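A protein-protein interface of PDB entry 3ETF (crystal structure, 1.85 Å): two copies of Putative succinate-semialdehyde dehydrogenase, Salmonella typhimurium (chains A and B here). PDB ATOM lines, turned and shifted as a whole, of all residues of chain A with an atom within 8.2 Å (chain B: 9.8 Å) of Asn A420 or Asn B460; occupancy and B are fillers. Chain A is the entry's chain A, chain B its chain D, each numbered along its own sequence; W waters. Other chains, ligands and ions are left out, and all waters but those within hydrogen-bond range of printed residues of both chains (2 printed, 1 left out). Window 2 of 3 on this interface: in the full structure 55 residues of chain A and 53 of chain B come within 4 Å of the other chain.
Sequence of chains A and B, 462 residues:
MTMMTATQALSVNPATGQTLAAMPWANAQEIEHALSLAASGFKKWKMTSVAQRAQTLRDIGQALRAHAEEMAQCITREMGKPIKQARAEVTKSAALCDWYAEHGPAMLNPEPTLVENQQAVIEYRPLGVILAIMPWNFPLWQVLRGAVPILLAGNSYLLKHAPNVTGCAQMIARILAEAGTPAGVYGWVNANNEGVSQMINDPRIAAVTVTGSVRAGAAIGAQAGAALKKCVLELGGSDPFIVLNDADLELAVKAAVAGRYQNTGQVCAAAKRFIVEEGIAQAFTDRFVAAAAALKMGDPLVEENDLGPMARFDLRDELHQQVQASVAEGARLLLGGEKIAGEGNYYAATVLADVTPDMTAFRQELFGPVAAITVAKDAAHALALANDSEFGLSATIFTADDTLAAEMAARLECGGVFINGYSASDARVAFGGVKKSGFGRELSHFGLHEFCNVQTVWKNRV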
ATOM      1  N   PHE A 241       8.937  -7.787  19.045  1.00  0.00           N
ATOM      2  CA  PHE A 241       8.893  -9.147  18.512  1.00  0.00           C
ATOM      3  C   PHE A 241       9.001  -8.910  17.011  1.00  0.00           C
ATOM      4  O   PHE A 241       8.049  -8.421  16.378  1.00  0.00           O
ATOM      5  CB  PHE A 241       7.564  -9.781  18.934  1.00  0.00           C
ATOM      6  CG  PHE A 241       7.396 -11.232  18.546  1.00  0.00           C
ATOM      7  CD1 PHE A 241       7.347 -12.226  19.535  1.00  0.00           C
ATOM      8  CD2 PHE A 241       7.213 -11.597  17.196  1.00  0.00           C
ATOM      9  CE1 PHE A 241       7.113 -13.576  19.198  1.00  0.00           C
ATOM     10  CE2 PHE A 241       7.016 -12.941  16.832  1.00  0.00           C
ATOM     11  CZ  PHE A 241       6.966 -13.941  17.836  1.00  0.00           C
ATOM     12  N   ILE A 242      10.190  -9.168  16.478  1.00  0.00           N
ATOM     13  CA  ILE A 242      10.538  -8.842  15.086  1.00  0.00           C
ATOM     14  C   ILE A 242      10.307 -10.057  14.195  1.00  0.00           C
ATOM     15  O   ILE A 242      10.745 -11.168  14.512  1.00  0.00           O
ATOM     16  CB  ILE A 242      12.010  -8.391  14.959  1.00  0.00           C
ATOM     17  CG1 ILE A 242      12.242  -7.071  15.723  1.00  0.00           C
ATOM     18  CG2 ILE A 242      12.390  -8.253  13.475  1.00  0.00           C
ATOM     19  CD1 ILE A 242      13.740  -6.747  15.989  1.00  0.00           C
ATOM     20  N   VAL A 243       9.572  -9.857  13.103  1.00  0.00           N
ATOM     21  CA  VAL A 243       9.345 -10.936  12.149  1.00  0.00           C
ATOM     22  C   VAL A 243       9.824 -10.470  10.769  1.00  0.00           C
ATOM     23  O   VAL A 243       9.278  -9.509  10.226  1.00  0.00           O
ATOM     24  CB  VAL A 243       7.854 -11.337  12.070  1.00  0.00           C
ATOM     25  CG1 VAL A 243       7.681 -12.502  11.065  1.00  0.00           C
ATOM     26  CG2 VAL A 243       7.325 -11.730  13.461  1.00  0.00           C
ATOM     27  N   LEU A 244      10.843 -11.143  10.223  1.00  0.00           N
ATOM     28  CA  LEU A 244      11.388 -10.784   8.904  1.00  0.00           C
ATOM     29  C   LEU A 244      10.743 -11.631   7.797  1.00  0.00           C
ATOM     30  O   LEU A 244      10.094 -12.640   8.093  1.00  0.00           O
ATOM     31  CB  LEU A 244      12.935 -10.857   8.892  1.00  0.00           C
ATOM     32  CG  LEU A 244      13.639  -9.969   9.948  1.00  0.00           C
ATOM     33  CD1 LEU A 244      15.147  -9.985   9.761  1.00  0.00           C
ATOM     34  CD2 LEU A 244      13.157  -8.521   9.886  1.00  0.00           C
ATOM     35  N   ASP A 246      11.678 -13.773   5.706  1.00  0.00           N
ATOM     36  CA  ASP A 246      12.083 -15.178   5.594  1.00  0.00           C
ATOM     37  C   ASP A 246      11.784 -16.045   6.823  1.00  0.00           C
ATOM     38  O   ASP A 246      12.284 -17.169   6.920  1.00  0.00           O
ATOM     39  CB  ASP A 246      13.569 -15.280   5.224  1.00  0.00           C
ATOM     40  CG  ASP A 246      14.492 -14.699   6.288  1.00  0.00           C
ATOM     41  OD1 ASP A 246      14.006 -14.174   7.311  1.00  0.00           O
ATOM     42  OD2 ASP A 246      15.723 -14.752   6.098  1.00  0.00           O
ATOM     43  N   ALA A 247      10.970 -15.540   7.751  1.00  0.00           N
ATOM     44  CA  ALA A 247      10.607 -16.314   8.948  1.00  0.00           C
ATOM     45  C   ALA A 247       9.759 -17.554   8.624  1.00  0.00           C
ATOM     46  O   ALA A 247       9.114 -17.631   7.564  1.00  0.00           O
ATOM     47  CB  ALA A 247       9.825 -15.418   9.923  1.00  0.00           C
ATOM     48  N   ASP A 248       9.755 -18.533   9.535  1.00  0.00           N
ATOM     49  CA  ASP A 248       8.723 -19.565   9.497  1.00  0.00           C
ATOM     50  C   ASP A 248       7.497 -18.828  10.039  1.00  0.00           C
ATOM     51  O   ASP A 248       7.362 -18.639  11.258  1.00  0.00           O
ATOM     52  CB  ASP A 248       9.088 -20.753  10.403  1.00  0.00           C
ATOM     53  CG  ASP A 248       7.958 -21.781  10.552  1.00  0.00           C
ATOM     54  OD1 ASP A 248       6.764 -21.476  10.354  1.00  0.00           O
ATOM     55  OD2 ASP A 248       8.283 -22.940  10.912  1.00  0.00           O
ATOM     56  N   LEU A 251       5.081 -20.535  12.789  1.00  0.00           N
ATOM     57  CA  LEU A 251       5.739 -20.629  14.107  1.00  0.00           C
ATOM     58  C   LEU A 251       5.820 -19.221  14.739  1.00  0.00           C
ATOM     59  O   LEU A 251       5.552 -19.049  15.943  1.00  0.00           O
ATOM     60  CB  LEU A 251       7.133 -21.250  13.989  1.00  0.00           C
ATOM     61  CG  LEU A 251       7.854 -21.457  15.328  1.00  0.00           C
ATOM     62  CD1 LEU A 251       7.072 -22.375  16.309  1.00  0.00           C
ATOM     63  CD2 LEU A 251       9.300 -21.967  15.121  1.00  0.00           C
ATOM     64  N   ALA A 252       6.169 -18.227  13.922  1.00  0.00           N
ATOM     65  CA  ALA A 252       6.237 -16.846  14.410  1.00  0.00           C
ATOM     66  C   ALA A 252       4.876 -16.433  14.983  1.00  0.00           C
ATOM     67  O   ALA A 252       4.802 -15.804  16.031  1.00  0.00           O
ATOM     68  CB  ALA A 252       6.673 -15.883  13.313  1.00  0.00           C
ATOM     69  N   ALA A 255       4.155 -18.231  18.351  1.00  0.00           N
ATOM     70  CA  ALA A 255       4.978 -17.649  19.427  1.00  0.00           C
ATOM     71  C   ALA A 255       4.481 -16.237  19.770  1.00  0.00           C
ATOM     72  O   ALA A 255       4.503 -15.837  20.944  1.00  0.00           O
ATOM     73  CB  ALA A 255       6.444 -17.628  19.031  1.00  0.00           C
ATOM     74  N   ALA A 395      13.386  -9.508  23.982  1.00  0.00           N
ATOM     75  CA  ALA A 395      13.021  -9.287  22.584  1.00  0.00           C
ATOM     76  C   ALA A 395      13.016 -10.628  21.883  1.00  0.00           C
ATOM     77  O   ALA A 395      13.638 -11.579  22.359  1.00  0.00           O
ATOM     78  CB  ALA A 395      14.016  -8.352  21.905  1.00  0.00           C
ATOM     79  N   THR A 396      12.321 -10.694  20.747  1.00  0.00           N
ATOM     80  CA  THR A 396      12.268 -11.915  19.942  1.00  0.00           C
ATOM     81  C   THR A 396      12.554 -11.516  18.501  1.00  0.00           C
ATOM     82  O   THR A 396      12.152 -10.421  18.071  1.00  0.00           O
ATOM     83  CB  THR A 396      10.868 -12.550  20.019  1.00  0.00           C
ATOM     84  OG1 THR A 396      10.605 -12.921  21.376  1.00  0.00           O
ATOM     85  CG2 THR A 396      10.788 -13.828  19.113  1.00  0.00           C
ATOM     86  N   ILE A 397      13.268 -12.376  17.765  1.00  0.00           N
ATOM     87  CA  ILE A 397      13.513 -12.163  16.325  1.00  0.00           C
ATOM     88  C   ILE A 397      13.208 -13.480  15.628  1.00  0.00           C
ATOM     89  O   ILE A 397      13.761 -14.522  16.007  1.00  0.00           O
ATOM     90  CB  ILE A 397      14.985 -11.823  15.983  1.00  0.00           C
ATOM     91  CG1 ILE A 397      15.544 -10.699  16.857  1.00  0.00           C
ATOM     92  CG2 ILE A 397      15.119 -11.460  14.479  1.00  0.00           C
ATOM     93  CD1 ILE A 397      17.094 -10.583  16.758  1.00  0.00           C
ATOM     94  N   PHE A 398      12.371 -13.424  14.595  1.00  0.00           N
ATOM     95  CA  PHE A 398      12.089 -14.590  13.761  1.00  0.00           C
ATOM     96  C   PHE A 398      12.625 -14.319  12.366  1.00  0.00           C
ATOM     97  O   PHE A 398      12.226 -13.352  11.720  1.00  0.00           O
ATOM     98  CB  PHE A 398      10.590 -14.885  13.683  1.00  0.00           C
ATOM     99  CG  PHE A 398      10.122 -15.884  14.701  1.00  0.00           C
ATOM    100  CD1 PHE A 398       9.904 -15.501  16.019  1.00  0.00           C
ATOM    101  CD2 PHE A 398       9.950 -17.215  14.336  1.00  0.00           C
ATOM    102  CE1 PHE A 398       9.483 -16.429  16.972  1.00  0.00           C
ATOM    103  CE2 PHE A 398       9.527 -18.164  15.272  1.00  0.00           C
ATOM    104  CZ  PHE A 398       9.306 -17.771  16.601  1.00  0.00           C
ATOM    105  N   THR A 399      13.559 -15.157  11.935  1.00  0.00           N
ATOM    106  CA  THR A 399      14.158 -15.074  10.606  1.00  0.00           C
ATOM    107  C   THR A 399      14.945 -16.352  10.345  1.00  0.00           C
ATOM    108  O   THR A 399      15.503 -16.940  11.269  1.00  0.00           O
ATOM    109  CB  THR A 399      15.105 -13.851  10.449  1.00  0.00           C
ATOM    110  OG1 THR A 399      15.757 -13.898   9.166  1.00  0.00           O
ATOM    111  CG2 THR A 399      16.150 -13.809  11.551  1.00  0.00           C
ATOM    112  N   ALA A 400      14.998 -16.761   9.085  1.00  0.00           N
ATOM    113  CA  ALA A 400      15.785 -17.931   8.691  1.00  0.00           C
ATOM    114  C   ALA A 400      17.269 -17.588   8.633  1.00  0.00           C
ATOM    115  O   ALA A 400      18.106 -18.491   8.612  1.00  0.00           O
ATOM    116  CB  ALA A 400      15.303 -18.457   7.341  1.00  0.00           C
ATOM    117  N   ASP A 401      17.605 -16.297   8.604  1.00  0.00           N
ATOM    118  CA  ASP A 401      19.003 -15.856   8.476  1.00  0.00           C
ATOM    119  C   ASP A 401      19.719 -15.853   9.832  1.00  0.00           C
ATOM    120  O   ASP A 401      19.649 -14.883  10.596  1.00  0.00           O
ATOM    121  CB  ASP A 401      19.061 -14.495   7.775  1.00  0.00           C
ATOM    122  CG  ASP A 401      20.483 -14.058   7.412  1.00  0.00           C
ATOM    123  OD1 ASP A 401      21.470 -14.529   8.017  1.00  0.00           O
ATOM    124  OD2 ASP A 401      20.595 -13.182   6.525  1.00  0.00           O
ATOM    125  N   ASP A 402      20.423 -16.952  10.119  1.00  0.00           N
ATOM    126  CA  ASP A 402      21.012 -17.183  11.451  1.00  0.00           C
ATOM    127  C   ASP A 402      22.096 -16.201  11.836  1.00  0.00           C
ATOM    128  O   ASP A 402      22.203 -15.815  12.998  1.00  0.00           O
ATOM    129  CB  ASP A 402      21.563 -18.609  11.556  1.00  0.00           C
ATOM    130  CG  ASP A 402      20.491 -19.667  11.386  1.00  0.00           C
ATOM    131  OD1 ASP A 402      19.320 -19.449  11.808  1.00  0.00           O
ATOM    132  OD2 ASP A 402      20.828 -20.740  10.836  1.00  0.00           O
ATOM    133  N   ALA A 405      20.409 -12.810  12.572  1.00  0.00           N
ATOM    134  CA  ALA A 405      19.747 -12.851  13.882  1.00  0.00           C
ATOM    135  C   ALA A 405      20.755 -12.636  15.001  1.00  0.00           C
ATOM    136  O   ALA A 405      20.480 -11.919  15.960  1.00  0.00           O
ATOM    137  CB  ALA A 405      19.016 -14.189  14.074  1.00  0.00           C
ATOM    138  N   VAL A 417      17.310 -12.049  24.414  1.00  0.00           N
ATOM    139  CA  VAL A 417      16.920 -12.105  23.004  1.00  0.00           C
ATOM    140  C   VAL A 417      16.637 -13.559  22.636  1.00  0.00           C
ATOM    141  O   VAL A 417      17.516 -14.419  22.772  1.00  0.00           O
ATOM    142  CB  VAL A 417      18.013 -11.550  22.052  1.00  0.00           C
ATOM    143  CG1 VAL A 417      17.542 -11.661  20.585  1.00  0.00           C
ATOM    144  CG2 VAL A 417      18.332 -10.097  22.381  1.00  0.00           C
ATOM    145  N   PHE A 418      15.421 -13.806  22.179  1.00  0.00           N
ATOM    146  CA  PHE A 418      14.985 -15.143  21.738  1.00  0.00           C
ATOM    147  C   PHE A 418      14.917 -15.187  20.245  1.00  0.00           C
ATOM    148  O   PHE A 418      14.190 -14.398  19.641  1.00  0.00           O
ATOM    149  CB  PHE A 418      13.651 -15.481  22.395  1.00  0.00           C
ATOM    150  CG  PHE A 418      13.812 -15.697  23.856  1.00  0.00           C
ATOM    151  CD1 PHE A 418      13.959 -16.990  24.370  1.00  0.00           C
ATOM    152  CD2 PHE A 418      13.942 -14.603  24.716  1.00  0.00           C
ATOM    153  CE1 PHE A 418      14.173 -17.200  25.768  1.00  0.00           C
ATOM    154  CE2 PHE A 418      14.168 -14.814  26.113  1.00  0.00           C
ATOM    155  CZ  PHE A 418      14.290 -16.116  26.612  1.00  0.00           C
ATOM    156  N   ILE A 419      15.691 -16.096  19.657  1.00  0.00           N
ATOM    157  CA  ILE A 419      15.723 -16.259  18.208  1.00  0.00           C
ATOM    158  C   ILE A 419      14.900 -17.465  17.799  1.00  0.00           C
ATOM    159  O   ILE A 419      15.195 -18.587  18.227  1.00  0.00           O
ATOM    160  CB  ILE A 419      17.171 -16.422  17.709  1.00  0.00           C
ATOM    161  CG1 ILE A 419      17.988 -15.172  18.068  1.00  0.00           C
ATOM    162  CG2 ILE A 419      17.199 -16.634  16.168  1.00  0.00           C
ATOM    163  CD1 ILE A 419      19.499 -15.398  18.017  1.00  0.00           C
ATOM    164  N   ASN A 420      13.891 -17.238  16.960  1.00  0.00           N
ATOM    165  CA  ASN A 420      13.046 -18.336  16.426  1.00  0.00           C
ATOM    166  C   ASN A 420      12.496 -19.238  17.523  1.00  0.00           C
ATOM    167  O   ASN A 420      12.542 -20.469  17.425  1.00  0.00           O
ATOM    168  CB  ASN A 420      13.825 -19.137  15.381  1.00  0.00           C
ATOM    169  CG  ASN A 420      14.171 -18.313  14.159  1.00  0.00           C
ATOM    170  OD1 ASN A 420      13.379 -17.474  13.715  1.00  0.00           O
ATOM    171  ND2 ASN A 420      15.357 -18.545  13.600  1.00  0.00           N
ATOM    172  N   GLY A 421      11.995 -18.611  18.591  1.00  0.00           N
ATOM    173  CA  GLY A 421      11.428 -19.344  19.706  1.00  0.00           C
ATOM    174  C   GLY A 421      10.565 -18.493  20.606  1.00  0.00           C
ATOM    175  O   GLY A 421      10.228 -17.350  20.271  1.00  0.00           O
ATOM    176  N   TYR A 422      10.207 -19.084  21.747  1.00  0.00           N
ATOM    177  CA  TYR A 422       9.271 -18.510  22.689  1.00  0.00           C
ATOM    178  C   TYR A 422      10.023 -17.948  23.869  1.00  0.00           C
ATOM    179  O   TYR A 422      10.663 -18.706  24.604  1.00  0.00           O
ATOM    180  CB  TYR A 422       8.363 -19.617  23.239  1.00  0.00           C
ATOM    181  CG  TYR A 422       7.328 -20.188  22.296  1.00  0.00           C
ATOM    182  CD1 TYR A 422       5.979 -19.921  22.495  1.00  0.00           C
ATOM    183  CD2 TYR A 422       7.691 -21.028  21.232  1.00  0.00           C
ATOM    184  CE1 TYR A 422       5.011 -20.463  21.643  1.00  0.00           C
ATOM    185  CE2 TYR A 422       6.720 -21.568  20.364  1.00  0.00           C
ATOM    186  CZ  TYR A 422       5.394 -21.286  20.594  1.00  0.00           C
ATOM    187  OH  TYR A 422       4.424 -21.823  19.773  1.00  0.00           O
ATOM    188  N   SER A 423       9.907 -16.640  24.125  1.00  0.00           N
ATOM    189  CA  SER A 423      10.605 -16.076  25.289  1.00  0.00           C
ATOM    190  C   SER A 423       9.984 -16.558  26.609  1.00  0.00           C
ATOM    191  O   SER A 423       8.768 -16.806  26.703  1.00  0.00           O
ATOM    192  CB  SER A 423      10.615 -14.540  25.251  1.00  0.00           C
ATOM    193  OG  SER A 423       9.289 -14.076  25.200  1.00  0.00           O
ATOM    194  N   VAL B 115      21.350 -24.949  29.529  1.00  0.00           N
ATOM    195  CA  VAL B 115      20.364 -25.285  28.490  1.00  0.00           C
ATOM    196  C   VAL B 115      21.051 -26.285  27.561  1.00  0.00           C
ATOM    197  O   VAL B 115      22.218 -26.112  27.195  1.00  0.00           O
ATOM    198  CB  VAL B 115      19.879 -24.029  27.734  1.00  0.00           C
ATOM    199  CG1 VAL B 115      18.971 -24.399  26.579  1.00  0.00           C
ATOM    200  CG2 VAL B 115      19.158 -23.088  28.720  1.00  0.00           C
ATOM    201  N   GLU B 116      20.354 -27.363  27.221  1.00  0.00           N
ATOM    202  CA  GLU B 116      21.011 -28.416  26.435  1.00  0.00           C
ATOM    203  C   GLU B 116      21.410 -27.991  25.034  1.00  0.00           C
ATOM    204  O   GLU B 116      20.768 -27.137  24.413  1.00  0.00           O
ATOM    205  CB  GLU B 116      20.097 -29.645  26.348  1.00  0.00           C
ATOM    206  CG  GLU B 116      19.939 -30.314  27.695  1.00  0.00           C
ATOM    207  CD  GLU B 116      18.873 -31.407  27.711  1.00  0.00           C
ATOM    208  OE1 GLU B 116      18.446 -31.876  26.624  1.00  0.00           O
ATOM    209  OE2 GLU B 116      18.479 -31.800  28.839  1.00  0.00           O
ATOM    210  N   ASN B 117      22.489 -28.601  24.546  1.00  0.00           N
ATOM    211  CA  ASN B 117      22.883 -28.524  23.142  1.00  0.00           C
ATOM    212  C   ASN B 117      23.265 -27.130  22.623  1.00  0.00           C
ATOM    213  O   ASN B 117      22.980 -26.795  21.477  1.00  0.00           O
ATOM    214  CB  ASN B 117      21.830 -29.189  22.236  1.00  0.00           C
ATOM    215  CG  ASN B 117      22.392 -29.580  20.880  1.00  0.00           C
ATOM    216  OD1 ASN B 117      23.554 -29.939  20.775  1.00  0.00           O
ATOM    217  ND2 ASN B 117      21.578 -29.500  19.837  1.00  0.00           N
ATOM    218  N   GLN B 118      23.901 -26.344  23.498  1.00  0.00           N
ATOM    219  CA  GLN B 118      24.450 -25.032  23.156  1.00  0.00           C
ATOM    220  C   GLN B 118      23.401 -24.128  22.504  1.00  0.00           C
ATOM    221  O   GLN B 118      23.710 -23.413  21.541  1.00  0.00           O
ATOM    222  CB  GLN B 118      25.683 -25.189  22.237  1.00  0.00           C
ATOM    223  CG  GLN B 118      26.844 -25.966  22.869  1.00  0.00           C
ATOM    224  CD  GLN B 118      26.630 -27.477  22.874  1.00  0.00           C
ATOM    225  OE1 GLN B 118      26.278 -28.063  21.854  1.00  0.00           O
ATOM    226  NE2 GLN B 118      26.868 -28.113  24.014  1.00  0.00           N
ATOM    227  N   GLN B 119      22.161 -24.173  23.010  1.00  0.00           N
ATOM    228  CA  GLN B 119      21.092 -23.322  22.458  1.00  0.00           C
ATOM    229  C   GLN B 119      21.020 -21.944  23.109  1.00  0.00           C
ATOM    230  O   GLN B 119      20.413 -21.033  22.533  1.00  0.00           O
ATOM    231  CB  GLN B 119      19.713 -24.008  22.576  1.00  0.00           C
ATOM    232  CG  GLN B 119      19.678 -25.379  21.854  1.00  0.00           C
ATOM    233  CD  GLN B 119      19.819 -25.238  20.343  1.00  0.00           C
ATOM    234  OE1 GLN B 119      20.901 -25.473  19.761  1.00  0.00           O
ATOM    235  NE2 GLN B 119      18.739 -24.869  19.698  1.00  0.00           N
ATOM    236  N   ALA B 120      21.609 -21.791  24.290  1.00  0.00           N
ATOM    237  CA  ALA B 120      21.569 -20.493  25.000  1.00  0.00           C
ATOM    238  C   ALA B 120      22.933 -20.117  25.554  1.00  0.00           C
ATOM    239  O   ALA B 120      23.666 -20.974  26.086  1.00  0.00           O
ATOM    240  CB  ALA B 120      20.558 -20.516  26.143  1.00  0.00           C
ATOM    241  N   VAL B 457      21.057 -14.951  25.257  1.00  0.00           N
ATOM    242  CA  VAL B 457      20.659 -15.144  23.826  1.00  0.00           C
ATOM    243  C   VAL B 457      20.317 -16.629  23.669  1.00  0.00           C
ATOM    244  O   VAL B 457      21.188 -17.481  23.852  1.00  0.00           O
ATOM    245  CB  VAL B 457      21.742 -14.730  22.800  1.00  0.00           C
ATOM    246  CG1 VAL B 457      21.209 -14.900  21.339  1.00  0.00           C
ATOM    247  CG2 VAL B 457      22.221 -13.268  23.033  1.00  0.00           C
ATOM    248  N   TRP B 458      19.059 -16.927  23.349  1.00  0.00           N
ATOM    249  CA  TRP B 458      18.566 -18.316  23.350  1.00  0.00           C
ATOM    250  C   TRP B 458      17.877 -18.560  22.025  1.00  0.00           C
ATOM    251  O   TRP B 458      16.885 -17.899  21.709  1.00  0.00           O
ATOM    252  CB  TRP B 458      17.550 -18.461  24.475  1.00  0.00           C
ATOM    253  CG  TRP B 458      17.145 -19.879  24.814  1.00  0.00           C
ATOM    254  CD1 TRP B 458      17.157 -20.973  23.992  1.00  0.00           C
ATOM    255  CD2 TRP B 458      16.622 -20.308  26.058  1.00  0.00           C
ATOM    256  NE1 TRP B 458      16.693 -22.086  24.680  1.00  0.00           N
ATOM    257  CE2 TRP B 458      16.361 -21.694  25.953  1.00  0.00           C
ATOM    258  CE3 TRP B 458      16.373 -19.651  27.282  1.00  0.00           C
ATOM    259  CZ2 TRP B 458      15.828 -22.443  27.019  1.00  0.00           C
ATOM    260  CZ3 TRP B 458      15.855 -20.392  28.338  1.00  0.00           C
ATOM    261  CH2 TRP B 458      15.598 -21.779  28.198  1.00  0.00           C
ATOM    262  N   LYS B 459      18.401 -19.499  21.238  1.00  0.00           N
ATOM    263  CA  LYS B 459      17.795 -19.807  19.956  1.00  0.00           C
ATOM    264  C   LYS B 459      16.927 -21.072  20.044  1.00  0.00           C
ATOM    265  O   LYS B 459      17.207 -21.968  20.858  1.00  0.00           O
ATOM    266  CB  LYS B 459      18.900 -19.965  18.896  1.00  0.00           C
ATOM    267  CG  LYS B 459      19.843 -21.142  19.148  1.00  0.00           C
ATOM    268  CD  LYS B 459      20.919 -21.194  18.041  1.00  0.00           C
ATOM    269  CE  LYS B 459      21.864 -22.368  18.215  1.00  0.00           C
ATOM    270  NZ  LYS B 459      22.811 -22.453  17.044  1.00  0.00           N
ATOM    271  N   ASN B 460      15.862 -21.113  19.243  1.00  0.00           N
ATOM    272  CA  ASN B 460      15.030 -22.312  19.092  1.00  0.00           C
ATOM    273  C   ASN B 460      14.366 -22.803  20.379  1.00  0.00           C
ATOM    274  O   ASN B 460      14.228 -24.023  20.580  1.00  0.00           O
ATOM    275  CB  ASN B 460      15.878 -23.452  18.478  1.00  0.00           C
ATOM    276  CG  ASN B 460      16.674 -23.017  17.270  1.00  0.00           C
ATOM    277  OD1 ASN B 460      16.154 -22.359  16.371  1.00  0.00           O
ATOM    278  ND2 ASN B 460      17.958 -23.420  17.222  1.00  0.00           N
ATOM    279  N   ARG B 461      13.945 -21.886  21.258  1.00  0.00           N
ATOM    280  CA  ARG B 461      13.272 -22.314  22.485  1.00  0.00           C
ATOM    281  C   ARG B 461      11.821 -22.655  22.145  1.00  0.00           C
ATOM    282  O   ARG B 461      10.992 -21.777  21.943  1.00  0.00           O
ATOM    283  CB  ARG B 461      13.339 -21.252  23.585  1.00  0.00           C
ATOM    284  CG  ARG B 461      12.682 -21.753  24.866  1.00  0.00           C
ATOM    285  CD  ARG B 461      12.718 -20.771  26.056  1.00  0.00           C
ATOM    286  NE  ARG B 461      11.981 -21.383  27.163  1.00  0.00           N
ATOM    287  CZ  ARG B 461      10.650 -21.413  27.265  1.00  0.00           C
ATOM    288  NH1 ARG B 461       9.869 -20.804  26.356  1.00  0.00           N
ATOM    289  NH2 ARG B 461      10.093 -22.040  28.306  1.00  0.00           N
ATOM    290  N   VAL B 462      11.524 -23.942  22.056  1.00  0.00           N
ATOM    291  CA  VAL B 462      10.192 -24.369  21.648  1.00  0.00           C
ATOM    292  C   VAL B 462       9.844 -25.607  22.444  1.00  0.00           C
ATOM    293  O   VAL B 462       8.788 -25.666  23.109  1.00  0.00           O
ATOM    294  CB  VAL B 462      10.130 -24.728  20.143  1.00  0.00           C
ATOM    295  CG1 VAL B 462       8.706 -25.201  19.766  1.00  0.00           C
ATOM    296  CG2 VAL B 462      10.572 -23.560  19.253  1.00  0.00           C
ATOM    297  OXT VAL B 462      10.642 -26.567  22.425  1.00  0.00           O
HETATM  298  O   HOH W   1      17.259 -20.464  14.855  1.00  0.00           O
HETATM  299  O   HOH W   2      13.160 -22.630  15.723  1.00  0.00           O
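Of chain B, only Asn B460 (3.5 Å) comes within 4 Å of Asn A420. Asn B460 touches just these residues of chain A: Ile A419 (2.8 Å) and Asn A420 (3.5 Å). No residue of chain B comes within 4 Å of Phe A398. Of the printed residues of chain B, Phe A418 touches Trp B458 and Arg B461. Of the printed residues of chain A, Val B457 touches Val A417 (3.4 Å) and Ile A419 (3.8 Å). Printed residues of chain A within 4 Å of Lys B459: Ile A419. Of the printed residues of chain B, Ile A419 touches Val B457, Trp B458, Lys B459 and Asn B460. Of the printed residues of chain A, Arg B461 touches Phe A418 (3.9 Å), Gly A421 (3.3 Å) and Tyr A422 (2.8 Å). Ala A255 touches none of the printed residues of chain B. The nearest residue of chain B that does not touch Asn A420 is Val B462 (4.1 Å).
The backbone carbonyl oxygen (O) of Thr A399 lies within hydrogen-bond range of the side-chain amide nitrogen (ND2) of Asn A420 (2.8 Å). N of Asn A420 sits at hydrogen-bond distance from O of Ile A397 (2.9 Å). The side-chain amide nitrogen (NE2) of Gln B119 sits close to the side-chain amide nitrogen (ND2) of Asn B460, at 3.0 Å. N of Ile A397 sits at hydrogen-bond distance from O of Phe A418. The backbone carbonyl oxygen (O) of Gln B119 is in hydrogen-bond range of the backbone NH (N) of Lys B459 (2.8 Å). The backbone carbonyl oxygen of Ala A395 sits at hydrogen-bond distance from the backbone NH of Phe A418, 2.9 Å away.
No position is printed for both chains. Of the 11 pairs that touch across the chains among the printed residues, none has its exchanged pair printed and touching as well.
Water W1 bridges the side-chain amide oxygen (OD1) of Asn B460 (2.7 Å) and the side-chain amide nitrogen (ND2) of Asn A420 (3.0 Å). Water W2 lies within hydrogen-bond range of O of Asn A420 (2.8 Å) and OD1 of Asn B460 (3.1 Å).
Of the 26 printed residues of chain A, 6 touch a printed residue of chain B. Along chain A the printed residues that touch a printed residue of chain B span positions 417 to 422. Of the 12 printed residues of chain B, 5 touch a printed residue of chain A. Hydrophobic or aromatic side chains of chain B within 4 Å of the printed part of chain A: Val B457 and Trp B458.
O of Val A417 touches CA of Val B457, at 3.4 Å. Phe A418 touches Trp B458. Arg B461 touches Phe A418 (CD to CE1, 3.9 Å). Val B457 touches Ile A419 (CG1 to CD1, 3.8 Å). Ile A419 touches Lys B459. Asn B460 touches Asn A420 (CA to O, 3.5 Å). CA of Gly A421 touches O of Arg B461, 3.3 Å away.
O of Ile A419 lies within hydrogen-bond range of N of Asn B460. O of Trp B458 sits at hydrogen-bond distance from N of Ile A419. N of Trp B458 sits at hydrogen-bond distance from O of Val A417, at 3.0 Å. The backbone NH (N) of Tyr A422 is in hydrogen-bond range of the backbone carbonyl oxygen (O) of Arg B461, 2.8 Å away.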
